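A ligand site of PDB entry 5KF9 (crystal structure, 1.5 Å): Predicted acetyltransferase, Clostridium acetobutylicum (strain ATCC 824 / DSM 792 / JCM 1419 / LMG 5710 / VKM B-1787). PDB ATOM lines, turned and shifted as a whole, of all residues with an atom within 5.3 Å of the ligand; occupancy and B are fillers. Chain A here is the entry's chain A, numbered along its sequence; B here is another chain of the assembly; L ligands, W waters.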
ATOM      1  N   ILE A  20      21.289  -5.460 -28.774  1.00  0.00           N
ATOM      2  CA  ILE A  20      21.806  -6.831 -28.564  1.00  0.00           C
ATOM      3  C   ILE A  20      21.438  -7.749 -29.716  1.00  0.00           C
ATOM      4  O   ILE A  20      21.617  -8.975 -29.632  1.00  0.00           O
ATOM      5  CB  ILE A  20      21.365  -7.414 -27.218  1.00  0.00           C
ATOM      6  CG1 ILE A  20      19.862  -7.720 -27.194  1.00  0.00           C
ATOM      7  CG2 ILE A  20      21.803  -6.501 -26.080  1.00  0.00           C
ATOM      8  CD1 ILE A  20      19.423  -8.424 -25.947  1.00  0.00           C
ATOM      9  N   ILE A  78      12.854 -10.691 -13.433  1.00  0.00           N
ATOM     10  CA  ILE A  78      13.241  -9.736 -14.435  1.00  0.00           C
ATOM     11  C   ILE A  78      13.410 -10.488 -15.737  1.00  0.00           C
ATOM     12  O   ILE A  78      14.410 -11.199 -15.925  1.00  0.00           O
ATOM     13  CB  ILE A  78      14.492  -8.982 -14.050  1.00  0.00           C
ATOM     14  CG1 ILE A  78      14.424  -8.433 -12.581  1.00  0.00           C
ATOM     15  CG2 ILE A  78      14.816  -7.917 -15.115  1.00  0.00           C
ATOM     16  CD1 ILE A  78      13.244  -7.538 -12.313  1.00  0.00           C
ATOM     17  N   ASN A  79      12.439 -10.348 -16.596  1.00  0.00           N
ATOM     18  CA  ASN A  79      12.445 -11.021 -17.888  1.00  0.00           C
ATOM     19  C   ASN A  79      13.557 -10.485 -18.785  1.00  0.00           C
ATOM     20  O   ASN A  79      14.279 -11.262 -19.438  1.00  0.00           O
ATOM     21  CB  ASN A  79      11.053 -10.932 -18.559  1.00  0.00           C
ATOM     22  CG  ASN A  79      11.080 -11.234 -20.052  1.00  0.00           C
ATOM     23  OD1 ASN A  79      11.468 -10.397 -20.886  1.00  0.00           O
ATOM     24  ND2 ASN A  79      10.687 -12.437 -20.399  1.00  0.00           N
ATOM     25  N   SER A  80      13.717  -9.175 -18.825  1.00  0.00           N
ATOM     26  CA  SER A  80      14.721  -8.523 -19.673  1.00  0.00           C
ATOM     27  C   SER A  80      14.792  -7.052 -19.242  1.00  0.00           C
ATOM     28  O   SER A  80      13.842  -6.496 -18.696  1.00  0.00           O
ATOM     29  CB  SER A  80      14.379  -8.615 -21.148  1.00  0.00           C
ATOM     30  OG  SER A  80      13.048  -8.162 -21.418  1.00  0.00           O
ATOM     31  N   ILE A  81      15.975  -6.472 -19.363  1.00  0.00           N
ATOM     32  CA  ILE A  81      16.149  -5.029 -19.171  1.00  0.00           C
ATOM     33  C   ILE A  81      17.217  -4.582 -20.168  1.00  0.00           C
ATOM     34  O   ILE A  81      18.270  -5.237 -20.272  1.00  0.00           O
ATOM     35  CB  ILE A  81      16.548  -4.692 -17.721  1.00  0.00           C
ATOM     36  CG1 ILE A  81      16.690  -3.178 -17.574  1.00  0.00           C
ATOM     37  CG2 ILE A  81      17.723  -5.465 -17.200  1.00  0.00           C
ATOM     38  CD1 ILE A  81      16.808  -2.734 -16.125  1.00  0.00           C
ATOM     39  N   ILE A  82      16.947  -3.521 -20.918  1.00  0.00           N
ATOM     40  CA  ILE A  82      17.877  -2.971 -21.879  1.00  0.00           C
ATOM     41  C   ILE A  82      17.746  -1.453 -21.800  1.00  0.00           C
ATOM     42  O   ILE A  82      16.630  -0.943 -21.871  1.00  0.00           O
ATOM     43  CB  ILE A  82      17.676  -3.447 -23.326  1.00  0.00           C
ATOM     44  CG1 ILE A  82      17.580  -4.963 -23.435  1.00  0.00           C
ATOM     45  CG2 ILE A  82      18.829  -2.922 -24.163  1.00  0.00           C
ATOM     46  CD1 ILE A  82      17.340  -5.482 -24.841  1.00  0.00           C
ATOM     47  N   VAL A  83      18.887  -0.788 -21.696  1.00  0.00           N
ATOM     48  CA  VAL A  83      18.999   0.659 -21.833  1.00  0.00           C
ATOM     49  C   VAL A  83      19.731   0.885 -23.144  1.00  0.00           C
ATOM     50  O   VAL A  83      20.772   0.259 -23.421  1.00  0.00           O
ATOM     51  CB  VAL A  83      19.736   1.263 -20.636  1.00  0.00           C
ATOM     52  CG1 VAL A  83      20.106   2.765 -20.843  1.00  0.00           C
ATOM     53  CG2 VAL A  83      18.845   1.128 -19.400  1.00  0.00           C
ATOM     54  N   PHE A  87      22.658   6.032 -24.067  1.00  0.00           N
ATOM     55  CA  PHE A  87      22.126   6.541 -22.807  1.00  0.00           C
ATOM     56  C   PHE A  87      22.532   5.754 -21.607  1.00  0.00           C
ATOM     57  O   PHE A  87      21.854   5.780 -20.605  1.00  0.00           O
ATOM     58  CB  PHE A  87      20.586   6.636 -22.866  1.00  0.00           C
ATOM     59  CG  PHE A  87      20.065   7.551 -23.982  1.00  0.00           C
ATOM     60  CD1 PHE A  87      19.833   8.902 -23.686  1.00  0.00           C
ATOM     61  CD2 PHE A  87      19.830   7.109 -25.244  1.00  0.00           C
ATOM     62  CE1 PHE A  87      19.379   9.756 -24.671  1.00  0.00           C
ATOM     63  CE2 PHE A  87      19.360   7.967 -26.245  1.00  0.00           C
ATOM     64  CZ  PHE A  87      19.132   9.295 -25.921  1.00  0.00           C
ATOM     65  N   ARG A  88      23.645   5.023 -21.708  1.00  0.00           N
ATOM     66  CA  ARG A  88      24.169   4.220 -20.591  1.00  0.00           C
ATOM     67  C   ARG A  88      24.872   5.062 -19.517  1.00  0.00           C
ATOM     68  O   ARG A  88      25.316   6.190 -19.830  1.00  0.00           O
ATOM     69  CB  ARG A  88      25.271   3.269 -21.135  1.00  0.00           C
ATOM     70  CG  ARG A  88      24.736   2.326 -22.191  1.00  0.00           C
ATOM     71  CD  ARG A  88      24.024   1.158 -21.538  1.00  0.00           C
ATOM     72  NE  ARG A  88      23.402   0.296 -22.557  1.00  0.00           N
ATOM     73  CZ  ARG A  88      24.017  -0.607 -23.305  1.00  0.00           C
ATOM     74  NH1 ARG A  88      23.326  -1.240 -24.233  1.00  0.00           N
ATOM     75  NH2 ARG A  88      25.278  -0.940 -23.062  1.00  0.00           N
ATOM     76  N   HIS A  89      24.987   4.518 -18.310  1.00  0.00           N
ATOM     77  CA  HIS A  89      25.708   5.118 -17.215  1.00  0.00           C
ATOM     78  C   HIS A  89      25.163   6.491 -16.928  1.00  0.00           C
ATOM     79  O   HIS A  89      25.910   7.350 -16.439  1.00  0.00           O
ATOM     80  CB  HIS A  89      27.184   5.140 -17.472  1.00  0.00           C
ATOM     81  CG  HIS A  89      27.787   3.784 -17.395  1.00  0.00           C
ATOM     82  ND1 HIS A  89      28.061   3.181 -16.194  1.00  0.00           N
ATOM     83  CD2 HIS A  89      28.170   2.910 -18.358  1.00  0.00           C
ATOM     84  CE1 HIS A  89      28.639   2.004 -16.418  1.00  0.00           C
ATOM     85  NE2 HIS A  89      28.683   1.816 -17.725  1.00  0.00           N
ATOM     86  N   GLN A  90      23.852   6.628 -17.069  1.00  0.00           N
ATOM     87  CA  GLN A  90      23.134   7.853 -16.687  1.00  0.00           C
ATOM     88  C   GLN A  90      22.114   7.505 -15.589  1.00  0.00           C
ATOM     89  O   GLN A  90      21.324   8.368 -15.212  1.00  0.00           O
ATOM     90  CB  GLN A  90      22.411   8.448 -17.897  1.00  0.00           C
ATOM     91  CG  GLN A  90      23.302   9.010 -18.972  1.00  0.00           C
ATOM     92  CD  GLN A  90      22.503   9.622 -20.133  1.00  0.00           C
ATOM     93  OE1 GLN A  90      21.326   9.996 -19.987  1.00  0.00           O
ATOM     94  NE2 GLN A  90      23.131   9.714 -21.287  1.00  0.00           N
ATOM     95  N   GLY A  91      22.134   6.293 -15.048  1.00  0.00           N
ATOM     96  CA  GLY A  91      21.222   5.911 -13.990  1.00  0.00           C
ATOM     97  C   GLY A  91      19.868   5.399 -14.451  1.00  0.00           C
ATOM     98  O   GLY A  91      19.023   5.068 -13.601  1.00  0.00           O
ATOM     99  N   ILE A  92      19.663   5.258 -15.754  1.00  0.00           N
ATOM    100  CA  ILE A  92      18.366   4.869 -16.285  1.00  0.00           C
ATOM    101  C   ILE A  92      18.056   3.410 -15.903  1.00  0.00           C
ATOM    102  O   ILE A  92      16.956   3.069 -15.488  1.00  0.00           O
ATOM    103  CB  ILE A  92      18.257   5.041 -17.788  1.00  0.00           C
ATOM    104  CG1 ILE A  92      18.466   6.522 -18.101  1.00  0.00           C
ATOM    105  CG2 ILE A  92      16.947   4.541 -18.315  1.00  0.00           C
ATOM    106  CD1 ILE A  92      18.645   6.840 -19.558  1.00  0.00           C
ATOM    107  N   GLY A  93      19.008   2.502 -16.043  1.00  0.00           N
ATOM    108  CA  GLY A  93      18.808   1.110 -15.670  1.00  0.00           C
ATOM    109  C   GLY A  93      18.466   0.973 -14.204  1.00  0.00           C
ATOM    110  O   GLY A  93      17.548   0.201 -13.831  1.00  0.00           O
ATOM    111  N   THR A  94      19.154   1.763 -13.352  1.00  0.00           N
ATOM    112  CA  THR A  94      18.832   1.797 -11.938  1.00  0.00           C
ATOM    113  C   THR A  94      17.410   2.256 -11.679  1.00  0.00           C
ATOM    114  O   THR A  94      16.683   1.613 -10.912  1.00  0.00           O
ATOM    115  CB  THR A  94      19.806   2.719 -11.189  1.00  0.00           C
ATOM    116  OG1 THR A  94      21.133   2.196 -11.307  1.00  0.00           O
ATOM    117  CG2 THR A  94      19.476   2.815  -9.712  1.00  0.00           C
ATOM    118  N   LYS A  95      16.976   3.293 -12.387  1.00  0.00           N
ATOM    119  CA  LYS A  95      15.615   3.823 -12.215  1.00  0.00           C
ATOM    120  C   LYS A  95      14.553   2.810 -12.669  1.00  0.00           C
ATOM    121  O   LYS A  95      13.548   2.594 -11.975  1.00  0.00           O
ATOM    122  CB  LYS A  95      15.447   5.186 -12.871  1.00  0.00           C
ATOM    123  CG  LYS A  95      16.065   6.292 -12.079  1.00  0.00           C
ATOM    124  CD  LYS A  95      15.905   7.575 -12.842  1.00  0.00           C
ATOM    125  CE  LYS A  95      16.183   8.747 -11.919  1.00  0.00           C
ATOM    126  NZ  LYS A  95      16.903   9.792 -12.683  1.00  0.00           N
ATOM    127  N   CYS A 114      16.779 -13.300 -12.236  1.00  0.00           N
ATOM    128  CA  CYS A 114      17.133 -12.800 -13.562  1.00  0.00           C
ATOM    129  C   CYS A 114      16.791 -13.851 -14.588  1.00  0.00           C
ATOM    130  O   CYS A 114      17.405 -14.949 -14.614  1.00  0.00           O
ATOM    131  CB  CYS A 114      18.635 -12.511 -13.671  1.00  0.00           C
ATOM    132  SG  CYS A 114      19.106 -11.057 -12.719  1.00  0.00           S
ATOM    133  N   GLY A 115      15.820 -13.588 -15.465  1.00  0.00           N
ATOM    134  CA  GLY A 115      15.348 -14.559 -16.418  1.00  0.00           C
ATOM    135  C   GLY A 115      14.737 -15.772 -15.730  1.00  0.00           C
ATOM    136  O   GLY A 115      14.399 -15.696 -14.538  1.00  0.00           O
ATOM    137  N   PHE A 122      15.467 -15.627 -21.638  1.00  0.00           N
ATOM    138  CA  PHE A 122      16.792 -16.042 -21.224  1.00  0.00           C
ATOM    139  C   PHE A 122      16.657 -16.960 -19.995  1.00  0.00           C
ATOM    140  O   PHE A 122      15.945 -16.605 -19.052  1.00  0.00           O
ATOM    141  CB  PHE A 122      17.637 -14.845 -20.795  1.00  0.00           C
ATOM    142  CG  PHE A 122      17.692 -13.740 -21.786  1.00  0.00           C
ATOM    143  CD1 PHE A 122      18.269 -13.972 -23.031  1.00  0.00           C
ATOM    144  CD2 PHE A 122      17.302 -12.488 -21.415  1.00  0.00           C
ATOM    145  CE1 PHE A 122      18.367 -12.901 -23.913  1.00  0.00           C
ATOM    146  CE2 PHE A 122      17.344 -11.444 -22.314  1.00  0.00           C
ATOM    147  CZ  PHE A 122      17.940 -11.681 -23.534  1.00  0.00           C
ATOM    148  N   GLY A 124      18.934 -17.207 -17.846  1.00  0.00           N
ATOM    149  CA  GLY A 124      19.680 -16.424 -16.856  1.00  0.00           C
ATOM    150  C   GLY A 124      20.391 -15.286 -17.554  1.00  0.00           C
ATOM    151  O   GLY A 124      20.022 -14.931 -18.654  1.00  0.00           O
ATOM    152  N   ILE A 125      21.354 -14.626 -16.915  1.00  0.00           N
ATOM    153  CA  ILE A 125      22.033 -13.512 -17.562  1.00  0.00           C
ATOM    154  C   ILE A 125      22.937 -14.062 -18.665  1.00  0.00           C
ATOM    155  O   ILE A 125      23.837 -14.847 -18.360  1.00  0.00           O
ATOM    156  CB  ILE A 125      22.904 -12.698 -16.547  1.00  0.00           C
ATOM    157  CG1 ILE A 125      22.015 -12.226 -15.384  1.00  0.00           C
ATOM    158  CG2 ILE A 125      23.653 -11.589 -17.272  1.00  0.00           C
ATOM    159  CD1 ILE A 125      22.874 -11.637 -14.262  1.00  0.00           C
ATOM    160  N   PRO A 126      22.720 -13.717 -19.944  1.00  0.00           N
ATOM    161  CA  PRO A 126      23.568 -14.275 -21.017  1.00  0.00           C
ATOM    162  C   PRO A 126      25.029 -13.913 -20.862  1.00  0.00           C
ATOM    163  O   PRO A 126      25.343 -12.818 -20.394  1.00  0.00           O
ATOM    164  CB  PRO A 126      23.012 -13.615 -22.287  1.00  0.00           C
ATOM    165  CG  PRO A 126      21.587 -13.271 -21.934  1.00  0.00           C
ATOM    166  CD  PRO A 126      21.652 -12.876 -20.482  1.00  0.00           C
ATOM    167  N   CYS A 129      25.987 -10.761 -22.126  1.00  0.00           N
ATOM    168  CA  CYS A 129      25.670  -9.644 -21.254  1.00  0.00           C
ATOM    169  C   CYS A 129      26.436  -9.768 -19.976  1.00  0.00           C
ATOM    170  O   CYS A 129      26.008  -9.245 -18.951  1.00  0.00           O
ATOM    171  CB  CYS A 129      24.164  -9.701 -20.938  1.00  0.00           C
ATOM    172  SG  CYS A 129      23.077  -9.465 -22.394  1.00  0.00           S
ATOM    173  N   PRO A 131      28.923  -8.093 -18.804  1.00  0.00           N
ATOM    174  CA  PRO A 131      29.137  -6.849 -18.074  1.00  0.00           C
ATOM    175  C   PRO A 131      27.962  -6.488 -17.156  1.00  0.00           C
ATOM    176  O   PRO A 131      28.189  -5.789 -16.140  1.00  0.00           O
ATOM    177  CB  PRO A 131      29.387  -5.807 -19.180  1.00  0.00           C
ATOM    178  CG  PRO A 131      29.966  -6.649 -20.311  1.00  0.00           C
ATOM    179  CD  PRO A 131      29.126  -7.913 -20.262  1.00  0.00           C
ATOM    180  N   SER A 132      26.747  -6.871 -17.491  1.00  0.00           N
ATOM    181  CA  SER A 132      25.576  -6.569 -16.676  1.00  0.00           C
ATOM    182  C   SER A 132      25.681  -7.301 -15.348  1.00  0.00           C
ATOM    183  O   SER A 132      24.961  -6.923 -14.410  1.00  0.00           O
ATOM    184  CB  SER A 132      24.242  -6.853 -17.374  1.00  0.00           C
ATOM    185  OG  SER A 132      24.002  -8.214 -17.407  1.00  0.00           O
ATOM    186  N   GLU A 134      27.841  -7.091 -13.111  1.00  0.00           N
ATOM    187  CA  GLU A 134      28.218  -6.099 -12.103  1.00  0.00           C
ATOM    188  C   GLU A 134      27.058  -5.179 -11.765  1.00  0.00           C
ATOM    189  O   GLU A 134      26.921  -4.780 -10.606  1.00  0.00           O
ATOM    190  CB  GLU A 134      29.400  -5.292 -12.612  1.00  0.00           C
ATOM    191  CG  GLU A 134      30.174  -4.559 -11.541  1.00  0.00           C
ATOM    192  CD  GLU A 134      30.622  -5.548 -10.462  1.00  0.00           C
ATOM    193  OE1 GLU A 134      31.257  -6.602 -10.787  1.00  0.00           O
ATOM    194  OE2 GLU A 134      30.296  -5.280  -9.296  1.00  0.00           O
ATOM    195  N   PHE A 135      26.255  -4.798 -12.760  1.00  0.00           N
ATOM    196  CA  PHE A 135      25.054  -3.989 -12.527  1.00  0.00           C
ATOM    197  C   PHE A 135      24.139  -4.718 -11.536  1.00  0.00           C
ATOM    198  O   PHE A 135      23.627  -4.133 -10.571  1.00  0.00           O
ATOM    199  CB  PHE A 135      24.363  -3.696 -13.854  1.00  0.00           C
ATOM    200  CG  PHE A 135      22.958  -3.144 -13.728  1.00  0.00           C
ATOM    201  CD1 PHE A 135      22.725  -1.792 -13.495  1.00  0.00           C
ATOM    202  CD2 PHE A 135      21.881  -3.944 -13.963  1.00  0.00           C
ATOM    203  CE1 PHE A 135      21.452  -1.311 -13.410  1.00  0.00           C
ATOM    204  CE2 PHE A 135      20.594  -3.450 -13.862  1.00  0.00           C
ATOM    205  CZ  PHE A 135      20.366  -2.109 -13.610  1.00  0.00           C
ATOM    206  N   PHE A 136      23.921  -5.997 -11.738  1.00  0.00           N
ATOM    207  CA  PHE A 136      23.049  -6.753 -10.850  1.00  0.00           C
ATOM    208  C   PHE A 136      23.708  -6.968  -9.482  1.00  0.00           C
ATOM    209  O   PHE A 136      23.013  -6.876  -8.478  1.00  0.00           O
ATOM    210  CB  PHE A 136      22.617  -8.061 -11.514  1.00  0.00           C
ATOM    211  CG  PHE A 136      21.649  -7.863 -12.643  1.00  0.00           C
ATOM    212  CD1 PHE A 136      20.354  -7.484 -12.435  1.00  0.00           C
ATOM    213  CD2 PHE A 136      22.063  -8.106 -13.973  1.00  0.00           C
ATOM    214  CE1 PHE A 136      19.469  -7.328 -13.489  1.00  0.00           C
ATOM    215  CE2 PHE A 136      21.201  -7.926 -15.011  1.00  0.00           C
ATOM    216  CZ  PHE A 136      19.905  -7.577 -14.785  1.00  0.00           C
ATOM    217  N   VAL A 138      25.689  -4.941  -7.881  1.00  0.00           N
ATOM    218  CA  VAL A 138      25.577  -3.694  -7.095  1.00  0.00           C
ATOM    219  C   VAL A 138      24.232  -3.655  -6.420  1.00  0.00           C
ATOM    220  O   VAL A 138      24.094  -3.131  -5.311  1.00  0.00           O
ATOM    221  CB  VAL A 138      25.789  -2.464  -7.999  1.00  0.00           C
ATOM    222  CG1 VAL A 138      25.332  -1.143  -7.344  1.00  0.00           C
ATOM    223  CG2 VAL A 138      27.255  -2.363  -8.424  1.00  0.00           C
ATOM    224  N   ASN B 295      34.494  -3.477 -21.016  1.00  0.00           N
ATOM    225  CA  ASN B 295      33.634  -2.310 -20.996  1.00  0.00           C
ATOM    226  C   ASN B 295      34.162  -1.165 -21.876  1.00  0.00           C
ATOM    227  O   ASN B 295      33.360  -0.376 -22.424  1.00  0.00           O
ATOM    228  CB  ASN B 295      33.420  -1.829 -19.559  1.00  0.00           C
ATOM    229  CG  ASN B 295      32.402  -2.620 -18.785  1.00  0.00           C
ATOM    230  OD1 ASN B 295      31.449  -3.161 -19.351  1.00  0.00           O
ATOM    231  ND2 ASN B 295      32.547  -2.610 -17.476  1.00  0.00           N
HETATM  232  N1  LIG L   1      29.957  -2.799 -15.921  1.00  0.00           N
HETATM  233  C1  LIG L   1      30.117  -2.638 -14.601  1.00  0.00           C
HETATM  234  N2  LIG L   1      29.197  -2.055 -13.808  1.00  0.00           N
HETATM  235  C2  LIG L   1      28.102  -1.546 -14.394  1.00  0.00           C
HETATM  236  C3  LIG L   1      27.829  -1.708 -15.815  1.00  0.00           C
HETATM  237  C4  LIG L   1      28.882  -2.353 -16.596  1.00  0.00           C
HETATM  238  N3  LIG L   1      28.738  -2.495 -17.940  1.00  0.00           N
HETATM  239  N4  LIG L   1      26.665  -1.089 -16.059  1.00  0.00           N
HETATM  240  C5  LIG L   1      26.169  -0.658 -14.862  1.00  0.00           C
HETATM  241  N5  LIG L   1      27.030  -0.939 -13.887  1.00  0.00           N
HETATM  242  C6  LIG L   1      26.947  -0.623 -12.437  1.00  0.00           C
HETATM  243  C7  LIG L   1      27.800   0.617 -12.133  1.00  0.00           C
HETATM  244  O1  LIG L   1      28.114   0.555 -10.761  1.00  0.00           O
HETATM  245  C8  LIG L   1      26.859   1.751 -12.439  1.00  0.00           C
HETATM  246  O2  LIG L   1      27.264   2.983 -11.806  1.00  0.00           O
HETATM  247  P1  LIG L   1      28.343   3.914 -12.586  1.00  0.00           P
HETATM  248  O3  LIG L   1      27.684   4.504 -13.765  1.00  0.00           O
HETATM  249  O4  LIG L   1      28.578   4.873 -11.406  1.00  0.00           O
HETATM  250  O5  LIG L   1      29.562   3.104 -12.921  1.00  0.00           O
HETATM  251  C9  LIG L   1      25.575   1.181 -11.849  1.00  0.00           C
HETATM  252  O6  LIG L   1      25.590  -0.229 -12.228  1.00  0.00           O
HETATM  253  C10 LIG L   1      24.349   1.874 -12.372  1.00  0.00           C
HETATM  254  O7  LIG L   1      24.178   1.760 -13.779  1.00  0.00           O
HETATM  255  P2  LIG L   1      23.085   2.513 -14.605  1.00  0.00           P
HETATM  256  O8  LIG L   1      23.596   3.777 -15.212  1.00  0.00           O
HETATM  257  O9  LIG L   1      21.825   2.549 -13.842  1.00  0.00           O
HETATM  258  O10 LIG L   1      22.951   1.345 -15.766  1.00  0.00           O
HETATM  259  P3  LIG L   1      22.560   1.573 -17.275  1.00  0.00           P
HETATM  260  O11 LIG L   1      21.497   2.557 -17.493  1.00  0.00           O
HETATM  261  O12 LIG L   1      23.802   1.880 -18.060  1.00  0.00           O
HETATM  262  O13 LIG L   1      21.951   0.144 -17.660  1.00  0.00           O
HETATM  263  C11 LIG L   1      22.156  -2.146 -18.292  1.00  0.00           C
HETATM  264  C12 LIG L   1      22.522  -1.091 -17.230  1.00  0.00           C
HETATM  265  C13 LIG L   1      20.627  -2.279 -18.357  1.00  0.00           C
HETATM  266  C14 LIG L   1      22.821  -3.447 -17.774  1.00  0.00           C
HETATM  267  C15 LIG L   1      22.781  -1.709 -19.609  1.00  0.00           C
HETATM  268  O14 LIG L   1      24.226  -1.780 -19.622  1.00  0.00           O
HETATM  269  C16 LIG L   1      22.286  -2.546 -20.773  1.00  0.00           C
HETATM  270  O15 LIG L   1      21.216  -2.392 -21.342  1.00  0.00           O
HETATM  271  N6  LIG L   1      23.108  -3.517 -21.204  1.00  0.00           N
HETATM  272  C17 LIG L   1      22.815  -4.422 -22.337  1.00  0.00           C
HETATM  273  C18 LIG L   1      21.656  -5.340 -22.091  1.00  0.00           C
HETATM  274  C19 LIG L   1      21.887  -6.180 -20.860  1.00  0.00           C
HETATM  275  O16 LIG L   1      22.975  -6.668 -20.608  1.00  0.00           O
HETATM  276  N7  LIG L   1      20.845  -6.431 -20.094  1.00  0.00           N
HETATM  277  C20 LIG L   1      20.772  -7.460 -19.078  1.00  0.00           C
HETATM  278  C21 LIG L   1      20.514  -8.862 -19.682  1.00  0.00           C
HETATM  279  S1  LIG L   1      20.079 -10.010 -18.389  1.00  0.00           S
HETATM  280  C22 LIG L   1      18.432  -9.809 -18.051  1.00  0.00           C
HETATM  281  O17 LIG L   1      17.919  -8.920 -18.706  1.00  0.00           O
HETATM  282  C23 LIG L   1      17.746 -10.644 -17.021  1.00  0.00           C
HETATM  283  O   HOH W   1      30.573   0.140 -18.768  1.00  0.00           O
HETATM  284  O   HOH W   2      25.106   5.360 -13.618  1.00  0.00           O
HETATM  285  O   HOH W   3      21.692   5.115 -17.973  1.00  0.00           O
HETATM  286  O   HOH W   4      25.776   0.086 -18.551  1.00  0.00           O
HETATM  287  O   HOH W   5      31.243  -5.521 -15.689  1.00  0.00           O
HETATM  288  O   HOH W   6      23.368   3.281  -9.743  1.00  0.00           O
HETATM  289  O   HOH W   7      25.737  -6.188 -20.832  1.00  0.00           O
HETATM  290  O   HOH W   8      27.078   7.107 -11.143  1.00  0.00           O
HETATM  291  O   HOH W   9      30.014  -1.039 -10.824  1.00  0.00           O
HETATM  292  O   HOH W  10      23.610  -1.363 -10.290  1.00  0.00           O
HETATM  293  O   HOH W  11      28.153   7.177 -14.430  1.00  0.00           O
HETATM  294  O   HOH W  12      26.272  -3.610 -20.162  1.00  0.00           O
HETATM  295  O   HOH W  13      31.318   2.298 -10.997  1.00  0.00           O
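N1 of the ligand sits close to O of Pro 131, at 3.5 Å. Ile 78 touches the ligand (O to C23, 3.6 Å). Ser 80 touches the ligand (CA to O17, 3.4 Å). Ile 82 touches the ligand. Arg 88 touches the ligand (CA to O12, 3.5 Å). N of Ile 92 touches O11 of the ligand, at 3.7 Å. Cys 114 touches the ligand. Gly 115 touches the ligand (N to C23, 3.8 Å). Pro 126 touches the ligand. Ser 132 touches the ligand. Glu 134 touches the ligand. CD1 of Phe 135 touches O6 of the ligand, 3.5 Å away. CG2 of Val 138 touches O1 of the ligand (3.8 Å). Hydrophobic or aromatic side chains within 4 Å of the ligand: Ile 81, Ile 82, Val 83, His 89, Pro 126, Pro 131, Phe 135 and Val 138. Of the 30 residues printed, 22 come within 4 Å of the ligand.
The backbone carbonyl oxygen of Val 83 is in hydrogen-bond range of the guanidinium group of Arg 88. The backbone carbonyl oxygen (O) of Cys 129 sits at hydrogen-bond distance from the side-chain hydroxyl (OG) of Ser 132 (2.7 Å). OG of Ser 80 lies within hydrogen-bond range of OD1 of Asn 79. N of Gly 115 is in hydrogen-bond range of O of Ile 78, 2.8 Å away.
Water W4 lies within hydrogen-bond range of an oxygen (O14) of the ligand (2.7 Å) and a ring nitrogen (NE2) of His 89 (3.5 Å). Water W2 lies within hydrogen-bond range of an oxygen (O8) of the ligand (2.7 Å) and the backbone NH (N) of Gly 91 (3.4 Å). Water W11 bridges O3 of the ligand (2.8 Å) and O of His 89 (3.0 Å). Water W10 bridges O of Phe 135 (2.8 Å) and O6 of the ligand (3.0 Å). Water W5 lies within hydrogen-bond range of a nitrogen (N1) of the ligand (3.0 Å) and the backbone carbonyl oxygen (O) of Pro 131 (3.1 Å). Water W1 lies within hydrogen-bond range of NE2 of His 89 (2.7 Å), N3 of the ligand (3.3 Å) and OD1 of Asn 295 of chain B (3.5 Å).
An oxygen (O9) of the ligand is in hydrogen-bond range of the backbone NH (N) of Thr 94 (2.8 Å). An oxygen (O9) of the ligand is in hydrogen-bond range of the side-chain hydroxyl (OG1) of Thr 94 (2.7 Å). N of His 89 is in hydrogen-bond range of O12 of the ligand, 2.9 Å away. O3 of the ligand sits at hydrogen-bond distance from ND1 of His 89, at 2.8 Å. The backbone NH of Ile 81 lies within hydrogen-bond range of an oxygen (O17) of the ligand (3.2 Å). The backbone carbonyl oxygen (O) of Ile 81 is in hydrogen-bond range of a nitrogen (N7) of the ligand (2.8 Å). An oxygen (O15) of the ligand is in hydrogen-bond range of the backbone NH of Val 83 (2.8 Å). An oxygen (O11) of the ligand lies within hydrogen-bond range of the backbone NH (N) of Gly 93, 2.9 Å away. N of Gly 91 lies within hydrogen-bond range of O8 of the ligand (2.9 Å). A nitrogen (N1) of the ligand sits at hydrogen-bond distance from the side-chain amide nitrogen (ND2) of Asn 295 of chain B, at 3.0 Å. SG of Cys 129 lies close to O16 of the ligand, at 3.3 Å. The backbone NH (N) of Gln 90 sits at hydrogen-bond distance from an oxygen (O8) of the ligand (3.4 Å).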
